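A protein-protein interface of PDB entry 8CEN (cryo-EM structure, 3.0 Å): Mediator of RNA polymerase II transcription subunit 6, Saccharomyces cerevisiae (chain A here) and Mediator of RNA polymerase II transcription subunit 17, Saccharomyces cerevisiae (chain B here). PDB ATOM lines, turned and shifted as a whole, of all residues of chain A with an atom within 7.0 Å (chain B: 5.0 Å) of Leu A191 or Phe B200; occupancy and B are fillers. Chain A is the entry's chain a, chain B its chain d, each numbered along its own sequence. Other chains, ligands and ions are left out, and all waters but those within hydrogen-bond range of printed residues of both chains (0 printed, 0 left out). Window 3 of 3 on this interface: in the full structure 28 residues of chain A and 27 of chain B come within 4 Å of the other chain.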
ATOM      1  N   LEU A 185     -20.325  27.622 -10.062  1.00  0.00           N
ATOM      2  CA  LEU A 185     -21.751  27.923 -10.120  1.00  0.00           C
ATOM      3  C   LEU A 185     -22.167  28.389 -11.509  1.00  0.00           C
ATOM      4  O   LEU A 185     -23.176  27.923 -12.043  1.00  0.00           O
ATOM      5  CB  LEU A 185     -22.106  28.975  -9.068  1.00  0.00           C
ATOM      6  CG  LEU A 185     -22.123  28.488  -7.617  1.00  0.00           C
ATOM      7  CD1 LEU A 185     -22.203  29.644  -6.642  1.00  0.00           C
ATOM      8  CD2 LEU A 185     -23.292  27.557  -7.411  1.00  0.00           C
ATOM      9  N   GLU A 186     -21.389  29.287 -12.121  1.00  0.00           N
ATOM     10  CA  GLU A 186     -21.756  29.806 -13.437  1.00  0.00           C
ATOM     11  C   GLU A 186     -21.667  28.722 -14.508  1.00  0.00           C
ATOM     12  O   GLU A 186     -22.566  28.596 -15.354  1.00  0.00           O
ATOM     13  CB  GLU A 186     -20.870  31.010 -13.779  1.00  0.00           C
ATOM     14  CG  GLU A 186     -21.275  31.815 -15.019  1.00  0.00           C
ATOM     15  CD  GLU A 186     -20.750  31.229 -16.318  1.00  0.00           C
ATOM     16  OE1 GLU A 186     -19.684  30.579 -16.284  1.00  0.00           O
ATOM     17  OE2 GLU A 186     -21.406  31.406 -17.366  1.00  0.00           O
ATOM     18  N   SER A 187     -20.608  27.910 -14.471  1.00  0.00           N
ATOM     19  CA  SER A 187     -20.478  26.823 -15.432  1.00  0.00           C
ATOM     20  C   SER A 187     -21.527  25.734 -15.219  1.00  0.00           C
ATOM     21  O   SER A 187     -21.911  25.056 -16.179  1.00  0.00           O
ATOM     22  CB  SER A 187     -19.066  26.255 -15.359  1.00  0.00           C
ATOM     23  OG  SER A 187     -18.808  25.790 -14.054  1.00  0.00           O
ATOM     24  N   LEU A 188     -21.999  25.542 -13.983  1.00  0.00           N
ATOM     25  CA  LEU A 188     -23.080  24.588 -13.757  1.00  0.00           C
ATOM     26  C   LEU A 188     -24.422  25.148 -14.210  1.00  0.00           C
ATOM     27  O   LEU A 188     -25.250  24.413 -14.763  1.00  0.00           O
ATOM     28  CB  LEU A 188     -23.136  24.186 -12.283  1.00  0.00           C
ATOM     29  CG  LEU A 188     -24.237  23.195 -11.891  1.00  0.00           C
ATOM     30  CD1 LEU A 188     -24.189  21.936 -12.743  1.00  0.00           C
ATOM     31  CD2 LEU A 188     -24.130  22.837 -10.423  1.00  0.00           C
ATOM     32  N   TYR A 189     -24.659  26.446 -13.988  1.00  0.00           N
ATOM     33  CA  TYR A 189     -25.902  27.052 -14.449  1.00  0.00           C
ATOM     34  C   TYR A 189     -25.962  27.142 -15.965  1.00  0.00           C
ATOM     35  O   TYR A 189     -27.059  27.237 -16.525  1.00  0.00           O
ATOM     36  CB  TYR A 189     -26.113  28.452 -13.869  1.00  0.00           C
ATOM     37  CG  TYR A 189     -26.402  28.506 -12.386  1.00  0.00           C
ATOM     38  CD1 TYR A 189     -27.266  27.595 -11.790  1.00  0.00           C
ATOM     39  CD2 TYR A 189     -25.768  29.434 -11.569  1.00  0.00           C
ATOM     40  CE1 TYR A 189     -27.527  27.644 -10.432  1.00  0.00           C
ATOM     41  CE2 TYR A 189     -26.020  29.488 -10.214  1.00  0.00           C
ATOM     42  CZ  TYR A 189     -26.895  28.588  -9.649  1.00  0.00           C
ATOM     43  OH  TYR A 189     -27.140  28.639  -8.296  1.00  0.00           O
ATOM     44  N   ASP A 190     -24.809  27.118 -16.638  1.00  0.00           N
ATOM     45  CA  ASP A 190     -24.813  26.986 -18.090  1.00  0.00           C
ATOM     46  C   ASP A 190     -25.314  25.623 -18.561  1.00  0.00           C
ATOM     47  O   ASP A 190     -25.647  25.479 -19.742  1.00  0.00           O
ATOM     48  CB  ASP A 190     -23.410  27.236 -18.643  1.00  0.00           C
ATOM     49  CG  ASP A 190     -23.421  27.616 -20.107  1.00  0.00           C
ATOM     50  OD1 ASP A 190     -23.663  28.802 -20.412  1.00  0.00           O
ATOM     51  OD2 ASP A 190     -23.201  26.725 -20.955  1.00  0.00           O
ATOM     52  N   LEU A 191     -25.379  24.629 -17.676  1.00  0.00           N
ATOM     53  CA  LEU A 191     -25.870  23.296 -18.002  1.00  0.00           C
ATOM     54  C   LEU A 191     -27.319  23.076 -17.586  1.00  0.00           C
ATOM     55  O   LEU A 191     -27.770  21.927 -17.539  1.00  0.00           O
ATOM     56  CB  LEU A 191     -24.980  22.236 -17.349  1.00  0.00           C
ATOM     57  CG  LEU A 191     -23.593  22.028 -17.955  1.00  0.00           C
ATOM     58  CD1 LEU A 191     -22.966  20.755 -17.421  1.00  0.00           C
ATOM     59  CD2 LEU A 191     -23.684  21.971 -19.469  1.00  0.00           C
ATOM     60  N   ILE A 192     -28.057  24.138 -17.277  1.00  0.00           N
ATOM     61  CA  ILE A 192     -29.409  24.038 -16.741  1.00  0.00           C
ATOM     62  C   ILE A 192     -30.409  24.417 -17.823  1.00  0.00           C
ATOM     63  O   ILE A 192     -30.291  25.478 -18.447  1.00  0.00           O
ATOM     64  CB  ILE A 192     -29.581  24.923 -15.493  1.00  0.00           C
ATOM     65  CG1 ILE A 192     -28.585  24.502 -14.419  1.00  0.00           C
ATOM     66  CG2 ILE A 192     -30.997  24.842 -14.962  1.00  0.00           C
ATOM     67  CD1 ILE A 192     -28.773  23.078 -13.967  1.00  0.00           C
ATOM     68  N   GLU A 193     -31.386  23.541 -18.047  1.00  0.00           N
ATOM     69  CA  GLU A 193     -32.507  23.799 -18.935  1.00  0.00           C
ATOM     70  C   GLU A 193     -33.799  23.668 -18.138  1.00  0.00           C
ATOM     71  O   GLU A 193     -33.945  22.761 -17.313  1.00  0.00           O
ATOM     72  CB  GLU A 193     -32.499  22.825 -20.129  1.00  0.00           C
ATOM     73  CG  GLU A 193     -33.784  22.780 -20.946  1.00  0.00           C
ATOM     74  CD  GLU A 193     -33.942  21.487 -21.723  1.00  0.00           C
ATOM     75  OE1 GLU A 193     -34.298  20.460 -21.106  1.00  0.00           O
ATOM     76  OE2 GLU A 193     -33.709  21.496 -22.950  1.00  0.00           O
ATOM     77  N   HIS A 201     -34.150  20.867 -14.666  1.00  0.00           N
ATOM     78  CA  HIS A 201     -33.267  19.710 -14.749  1.00  0.00           C
ATOM     79  C   HIS A 201     -32.075  20.054 -15.636  1.00  0.00           C
ATOM     80  O   HIS A 201     -31.852  21.216 -15.988  1.00  0.00           O
ATOM     81  CB  HIS A 201     -34.041  18.490 -15.265  1.00  0.00           C
ATOM     82  CG  HIS A 201     -34.594  18.669 -16.645  1.00  0.00           C
ATOM     83  ND1 HIS A 201     -35.708  19.437 -16.906  1.00  0.00           N
ATOM     84  CD2 HIS A 201     -34.187  18.179 -17.839  1.00  0.00           C
ATOM     85  CE1 HIS A 201     -35.962  19.414 -18.202  1.00  0.00           C
ATOM     86  NE2 HIS A 201     -35.054  18.657 -18.792  1.00  0.00           N
ATOM     87  N   TYR A 202     -31.308  19.030 -16.000  1.00  0.00           N
ATOM     88  CA  TYR A 202     -30.084  19.203 -16.767  1.00  0.00           C
ATOM     89  C   TYR A 202     -30.365  19.087 -18.258  1.00  0.00           C
ATOM     90  O   TYR A 202     -31.202  18.288 -18.685  1.00  0.00           O
ATOM     91  CB  TYR A 202     -29.037  18.165 -16.362  1.00  0.00           C
ATOM     92  CG  TYR A 202     -28.714  18.167 -14.889  1.00  0.00           C
ATOM     93  CD1 TYR A 202     -27.743  19.013 -14.372  1.00  0.00           C
ATOM     94  CD2 TYR A 202     -29.377  17.316 -14.015  1.00  0.00           C
ATOM     95  CE1 TYR A 202     -27.444  19.016 -13.025  1.00  0.00           C
ATOM     96  CE2 TYR A 202     -29.087  17.313 -12.669  1.00  0.00           C
ATOM     97  CZ  TYR A 202     -28.119  18.163 -12.178  1.00  0.00           C
ATOM     98  OH  TYR A 202     -27.826  18.160 -10.835  1.00  0.00           O
ATOM     99  N   LYS A 203     -29.653  19.890 -19.043  1.00  0.00           N
ATOM    100  CA  LYS A 203     -29.801  19.859 -20.491  1.00  0.00           C
ATOM    101  C   LYS A 203     -29.246  18.552 -21.048  1.00  0.00           C
ATOM    102  O   LYS A 203     -28.141  18.131 -20.694  1.00  0.00           O
ATOM    103  CB  LYS A 203     -29.083  21.053 -21.114  1.00  0.00           C
ATOM    104  CG  LYS A 203     -29.695  21.556 -22.411  1.00  0.00           C
ATOM    105  CD  LYS A 203     -29.074  22.879 -22.841  1.00  0.00           C
ATOM    106  CE  LYS A 203     -29.018  23.880 -21.695  1.00  0.00           C
ATOM    107  NZ  LYS A 203     -28.261  25.106 -22.065  1.00  0.00           N
ATOM    108  N   VAL A 204     -30.019  17.912 -21.920  1.00  0.00           N
ATOM    109  CA  VAL A 204     -29.641  16.633 -22.517  1.00  0.00           C
ATOM    110  C   VAL A 204     -28.701  16.884 -23.690  1.00  0.00           C
ATOM    111  O   VAL A 204     -29.040  17.663 -24.595  1.00  0.00           O
ATOM    112  CB  VAL A 204     -30.882  15.840 -22.960  1.00  0.00           C
ATOM    113  CG1 VAL A 204     -30.475  14.601 -23.743  1.00  0.00           C
ATOM    114  CG2 VAL A 204     -31.727  15.461 -21.754  1.00  0.00           C
ATOM    115  N   PRO A 205     -27.516  16.273 -23.710  1.00  0.00           N
ATOM    116  CA  PRO A 205     -26.614  16.449 -24.853  1.00  0.00           C
ATOM    117  C   PRO A 205     -27.163  15.807 -26.119  1.00  0.00           C
ATOM    118  O   PRO A 205     -27.912  14.829 -26.078  1.00  0.00           O
ATOM    119  CB  PRO A 205     -25.320  15.759 -24.400  1.00  0.00           C
ATOM    120  CG  PRO A 205     -25.456  15.575 -22.919  1.00  0.00           C
ATOM    121  CD  PRO A 205     -26.921  15.432 -22.660  1.00  0.00           C
ATOM    122  N   MET B 195     -26.706  22.176 -27.855  1.00  0.00           N
ATOM    123  CA  MET B 195     -25.625  21.793 -26.958  1.00  0.00           C
ATOM    124  C   MET B 195     -25.214  20.355 -27.248  1.00  0.00           C
ATOM    125  O   MET B 195     -26.068  19.479 -27.414  1.00  0.00           O
ATOM    126  CB  MET B 195     -26.065  21.966 -25.498  1.00  0.00           C
ATOM    127  CG  MET B 195     -25.024  21.670 -24.421  1.00  0.00           C
ATOM    128  SD  MET B 195     -24.798  19.942 -23.967  1.00  0.00           S
ATOM    129  CE  MET B 195     -26.310  19.649 -23.064  1.00  0.00           C
ATOM    130  N   THR B 196     -23.907  20.116 -27.296  1.00  0.00           N
ATOM    131  CA  THR B 196     -23.365  18.833 -27.716  1.00  0.00           C
ATOM    132  C   THR B 196     -22.566  18.183 -26.592  1.00  0.00           C
ATOM    133  O   THR B 196     -22.243  18.806 -25.577  1.00  0.00           O
ATOM    134  CB  THR B 196     -22.492  18.989 -28.968  1.00  0.00           C
ATOM    135  OG1 THR B 196     -22.049  17.699 -29.408  1.00  0.00           O
ATOM    136  CG2 THR B 196     -21.287  19.863 -28.672  1.00  0.00           C
ATOM    137  N   GLN B 197     -22.249  16.902 -26.811  1.00  0.00           N
ATOM    138  CA  GLN B 197     -21.621  16.069 -25.788  1.00  0.00           C
ATOM    139  C   GLN B 197     -20.218  16.552 -25.434  1.00  0.00           C
ATOM    140  O   GLN B 197     -19.835  16.542 -24.259  1.00  0.00           O
ATOM    141  CB  GLN B 197     -21.583  14.617 -26.267  1.00  0.00           C
ATOM    142  CG  GLN B 197     -21.013  13.624 -25.266  1.00  0.00           C
ATOM    143  CD  GLN B 197     -21.823  13.539 -23.988  1.00  0.00           C
ATOM    144  OE1 GLN B 197     -21.421  14.060 -22.950  1.00  0.00           O
ATOM    145  NE2 GLN B 197     -22.970  12.873 -24.058  1.00  0.00           N
ATOM    146  N   GLU B 198     -19.432  16.967 -26.430  1.00  0.00           N
ATOM    147  CA  GLU B 198     -18.058  17.390 -26.163  1.00  0.00           C
ATOM    148  C   GLU B 198     -18.011  18.721 -25.412  1.00  0.00           C
ATOM    149  O   GLU B 198     -17.194  18.896 -24.497  1.00  0.00           O
ATOM    150  CB  GLU B 198     -17.274  17.428 -27.480  1.00  0.00           C
ATOM    151  CG  GLU B 198     -17.887  18.274 -28.596  1.00  0.00           C
ATOM    152  CD  GLU B 198     -17.382  19.697 -28.612  1.00  0.00           C
ATOM    153  OE1 GLU B 198     -16.303  19.944 -28.040  1.00  0.00           O
ATOM    154  OE2 GLU B 198     -18.062  20.569 -29.193  1.00  0.00           O
ATOM    155  N   GLN B 199     -18.904  19.653 -25.752  1.00  0.00           N
ATOM    156  CA  GLN B 199     -19.004  20.895 -24.992  1.00  0.00           C
ATOM    157  C   GLN B 199     -19.509  20.627 -23.577  1.00  0.00           C
ATOM    158  O   GLN B 199     -19.025  21.232 -22.608  1.00  0.00           O
ATOM    159  CB  GLN B 199     -19.912  21.874 -25.735  1.00  0.00           C
ATOM    160  CG  GLN B 199     -19.884  23.296 -25.217  1.00  0.00           C
ATOM    161  CD  GLN B 199     -20.847  24.194 -25.969  1.00  0.00           C
ATOM    162  OE1 GLN B 199     -21.611  23.730 -26.816  1.00  0.00           O
ATOM    163  NE2 GLN B 199     -20.807  25.488 -25.672  1.00  0.00           N
ATOM    164  N   PHE B 200     -20.455  19.690 -23.445  1.00  0.00           N
ATOM    165  CA  PHE B 200     -20.950  19.280 -22.136  1.00  0.00           C
ATOM    166  C   PHE B 200     -19.838  18.696 -21.276  1.00  0.00           C
ATOM    167  O   PHE B 200     -19.723  19.026 -20.090  1.00  0.00           O
ATOM    168  CB  PHE B 200     -22.085  18.268 -22.318  1.00  0.00           C
ATOM    169  CG  PHE B 200     -22.523  17.594 -21.048  1.00  0.00           C
ATOM    170  CD1 PHE B 200     -23.371  18.237 -20.163  1.00  0.00           C
ATOM    171  CD2 PHE B 200     -22.117  16.300 -20.760  1.00  0.00           C
ATOM    172  CE1 PHE B 200     -23.784  17.613 -19.000  1.00  0.00           C
ATOM    173  CE2 PHE B 200     -22.525  15.671 -19.599  1.00  0.00           C
ATOM    174  CZ  PHE B 200     -23.360  16.328 -18.719  1.00  0.00           C
ATOM    175  N   VAL B 201     -18.991  17.847 -21.860  1.00  0.00           N
ATOM    176  CA  VAL B 201     -17.976  17.188 -21.050  1.00  0.00           C
ATOM    177  C   VAL B 201     -16.815  18.135 -20.741  1.00  0.00           C
ATOM    178  O   VAL B 201     -16.197  18.019 -19.676  1.00  0.00           O
ATOM    179  CB  VAL B 201     -17.503  15.872 -21.707  1.00  0.00           C
ATOM    180  CG1 VAL B 201     -16.636  16.116 -22.932  1.00  0.00           C
ATOM    181  CG2 VAL B 201     -16.783  14.987 -20.690  1.00  0.00           C
ATOM    182  N   LYS B 202     -16.519  19.117 -21.607  1.00  0.00           N
ATOM    183  CA  LYS B 202     -15.495  20.083 -21.209  1.00  0.00           C
ATOM    184  C   LYS B 202     -16.012  21.034 -20.133  1.00  0.00           C
ATOM    185  O   LYS B 202     -15.248  21.428 -19.241  1.00  0.00           O
ATOM    186  CB  LYS B 202     -14.930  20.869 -22.397  1.00  0.00           C
ATOM    187  CG  LYS B 202     -15.867  21.794 -23.137  1.00  0.00           C
ATOM    188  CD  LYS B 202     -15.095  22.515 -24.234  1.00  0.00           C
ATOM    189  CE  LYS B 202     -14.726  21.605 -25.385  1.00  0.00           C
ATOM    190  NZ  LYS B 202     -15.907  21.128 -26.121  1.00  0.00           N
ATOM    191  N   ARG B 203     -17.301  21.399 -20.175  1.00  0.00           N
ATOM    192  CA  ARG B 203     -17.861  22.164 -19.060  1.00  0.00           C
ATOM    193  C   ARG B 203     -17.860  21.344 -17.775  1.00  0.00           C
ATOM    194  O   ARG B 203     -17.568  21.875 -16.696  1.00  0.00           O
ATOM    195  CB  ARG B 203     -19.272  22.655 -19.377  1.00  0.00           C
ATOM    196  CG  ARG B 203     -19.310  24.025 -20.029  1.00  0.00           C
ATOM    197  CD  ARG B 203     -20.736  24.508 -20.182  1.00  0.00           C
ATOM    198  NE  ARG B 203     -21.473  23.759 -21.191  1.00  0.00           N
ATOM    199  CZ  ARG B 203     -21.846  24.249 -22.364  1.00  0.00           C
ATOM    200  NH1 ARG B 203     -21.572  25.494 -22.712  1.00  0.00           N
ATOM    201  NH2 ARG B 203     -22.525  23.473 -23.202  1.00  0.00           N
ATOM    202  N   ARG B 204     -18.156  20.044 -17.880  1.00  0.00           N
ATOM    203  CA  ARG B 204     -18.108  19.159 -16.721  1.00  0.00           C
ATOM    204  C   ARG B 204     -16.708  19.104 -16.124  1.00  0.00           C
ATOM    205  O   ARG B 204     -16.536  19.229 -14.905  1.00  0.00           O
ATOM    206  CB  ARG B 204     -18.563  17.754 -17.129  1.00  0.00           C
ATOM    207  CG  ARG B 204     -20.070  17.556 -17.143  1.00  0.00           C
ATOM    208  CD  ARG B 204     -20.595  17.236 -15.758  1.00  0.00           C
ATOM    209  NE  ARG B 204     -19.682  16.399 -14.989  1.00  0.00           N
ATOM    210  CZ  ARG B 204     -19.579  15.083 -15.124  1.00  0.00           C
ATOM    211  NH1 ARG B 204     -20.392  14.404 -15.916  1.00  0.00           N
ATOM    212  NH2 ARG B 204     -18.652  14.433 -14.429  1.00  0.00           N
ATOM    213  N   MET B 207     -15.704  22.610 -14.510  1.00  0.00           N
ATOM    214  CA  MET B 207     -16.330  22.876 -13.218  1.00  0.00           C
ATOM    215  C   MET B 207     -15.857  21.889 -12.159  1.00  0.00           C
ATOM    216  O   MET B 207     -15.768  22.252 -10.979  1.00  0.00           O
ATOM    217  CB  MET B 207     -17.856  22.889 -13.331  1.00  0.00           C
ATOM    218  CG  MET B 207     -18.574  21.614 -13.684  1.00  0.00           C
ATOM    219  SD  MET B 207     -20.329  22.032 -13.784  1.00  0.00           S
ATOM    220  CE  MET B 207     -21.061  20.464 -14.212  1.00  0.00           C
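Among the printed residues, pairs that only touch across the chains: Ser A187 with Met B207 (3.1 Å), Leu A191 with Arg B203 (3.3 Å), Lys A203 with Met B195 (3.4 Å), Leu A191 with Phe B200 (3.6 Å), Pro A205 with Met B195 (3.6 Å), Val A204 with Met B195 (3.7 Å), Pro A205 with Gln B197 (3.7 Å), Leu A191 with Met B207 (3.7 Å) and Leu A188 with Met B207 (3.8 Å).
The backbone carbonyl oxygen (O) of Leu A191 is in hydrogen-bond range of the backbone NH (N) of Lys A203 (3.2 Å). The side-chain amide nitrogen (NE2) of Gln B199 lies close to the guanidinium group (NH1) of Arg B203, 3.1 Å away.
The side-chain carboxylate of Asp A190 lies within salt-bridge range of the guanidinium group of Arg B203.
Leu A191 touches just these residues of chain B: Phe B200 (3.6 Å), Arg B203 (3.3 Å) and Met B207 (3.7 Å). Phe B200 touches just one residue of chain A: Leu A191 (3.6 Å). Of the printed residues of chain B, Pro A205 touches Met B195 (3.6 Å) and Gln B197 (3.7 Å). Printed residues of chain B within 4 Å of Lys A203: Met B195. Of the printed residues of chain B, Leu A188 touches Met B207. Printed residues of chain B within 4 Å of Ser A187: Met B207 (3.1 Å). Lys B202 touches none of the printed residues of chain A. The nearest printed residue of chain A that does not touch Gln B197 is Val A204 (7.0 Å).
Of the 14 printed residues of chain A, 7 touch a printed residue of chain B. Hydrophobic or aromatic side chains of chain A within 4 Å of the printed part of chain B: Leu A188, Leu A191 and Pro A205. Among the printed residues, 10 pairs touch across the chains.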
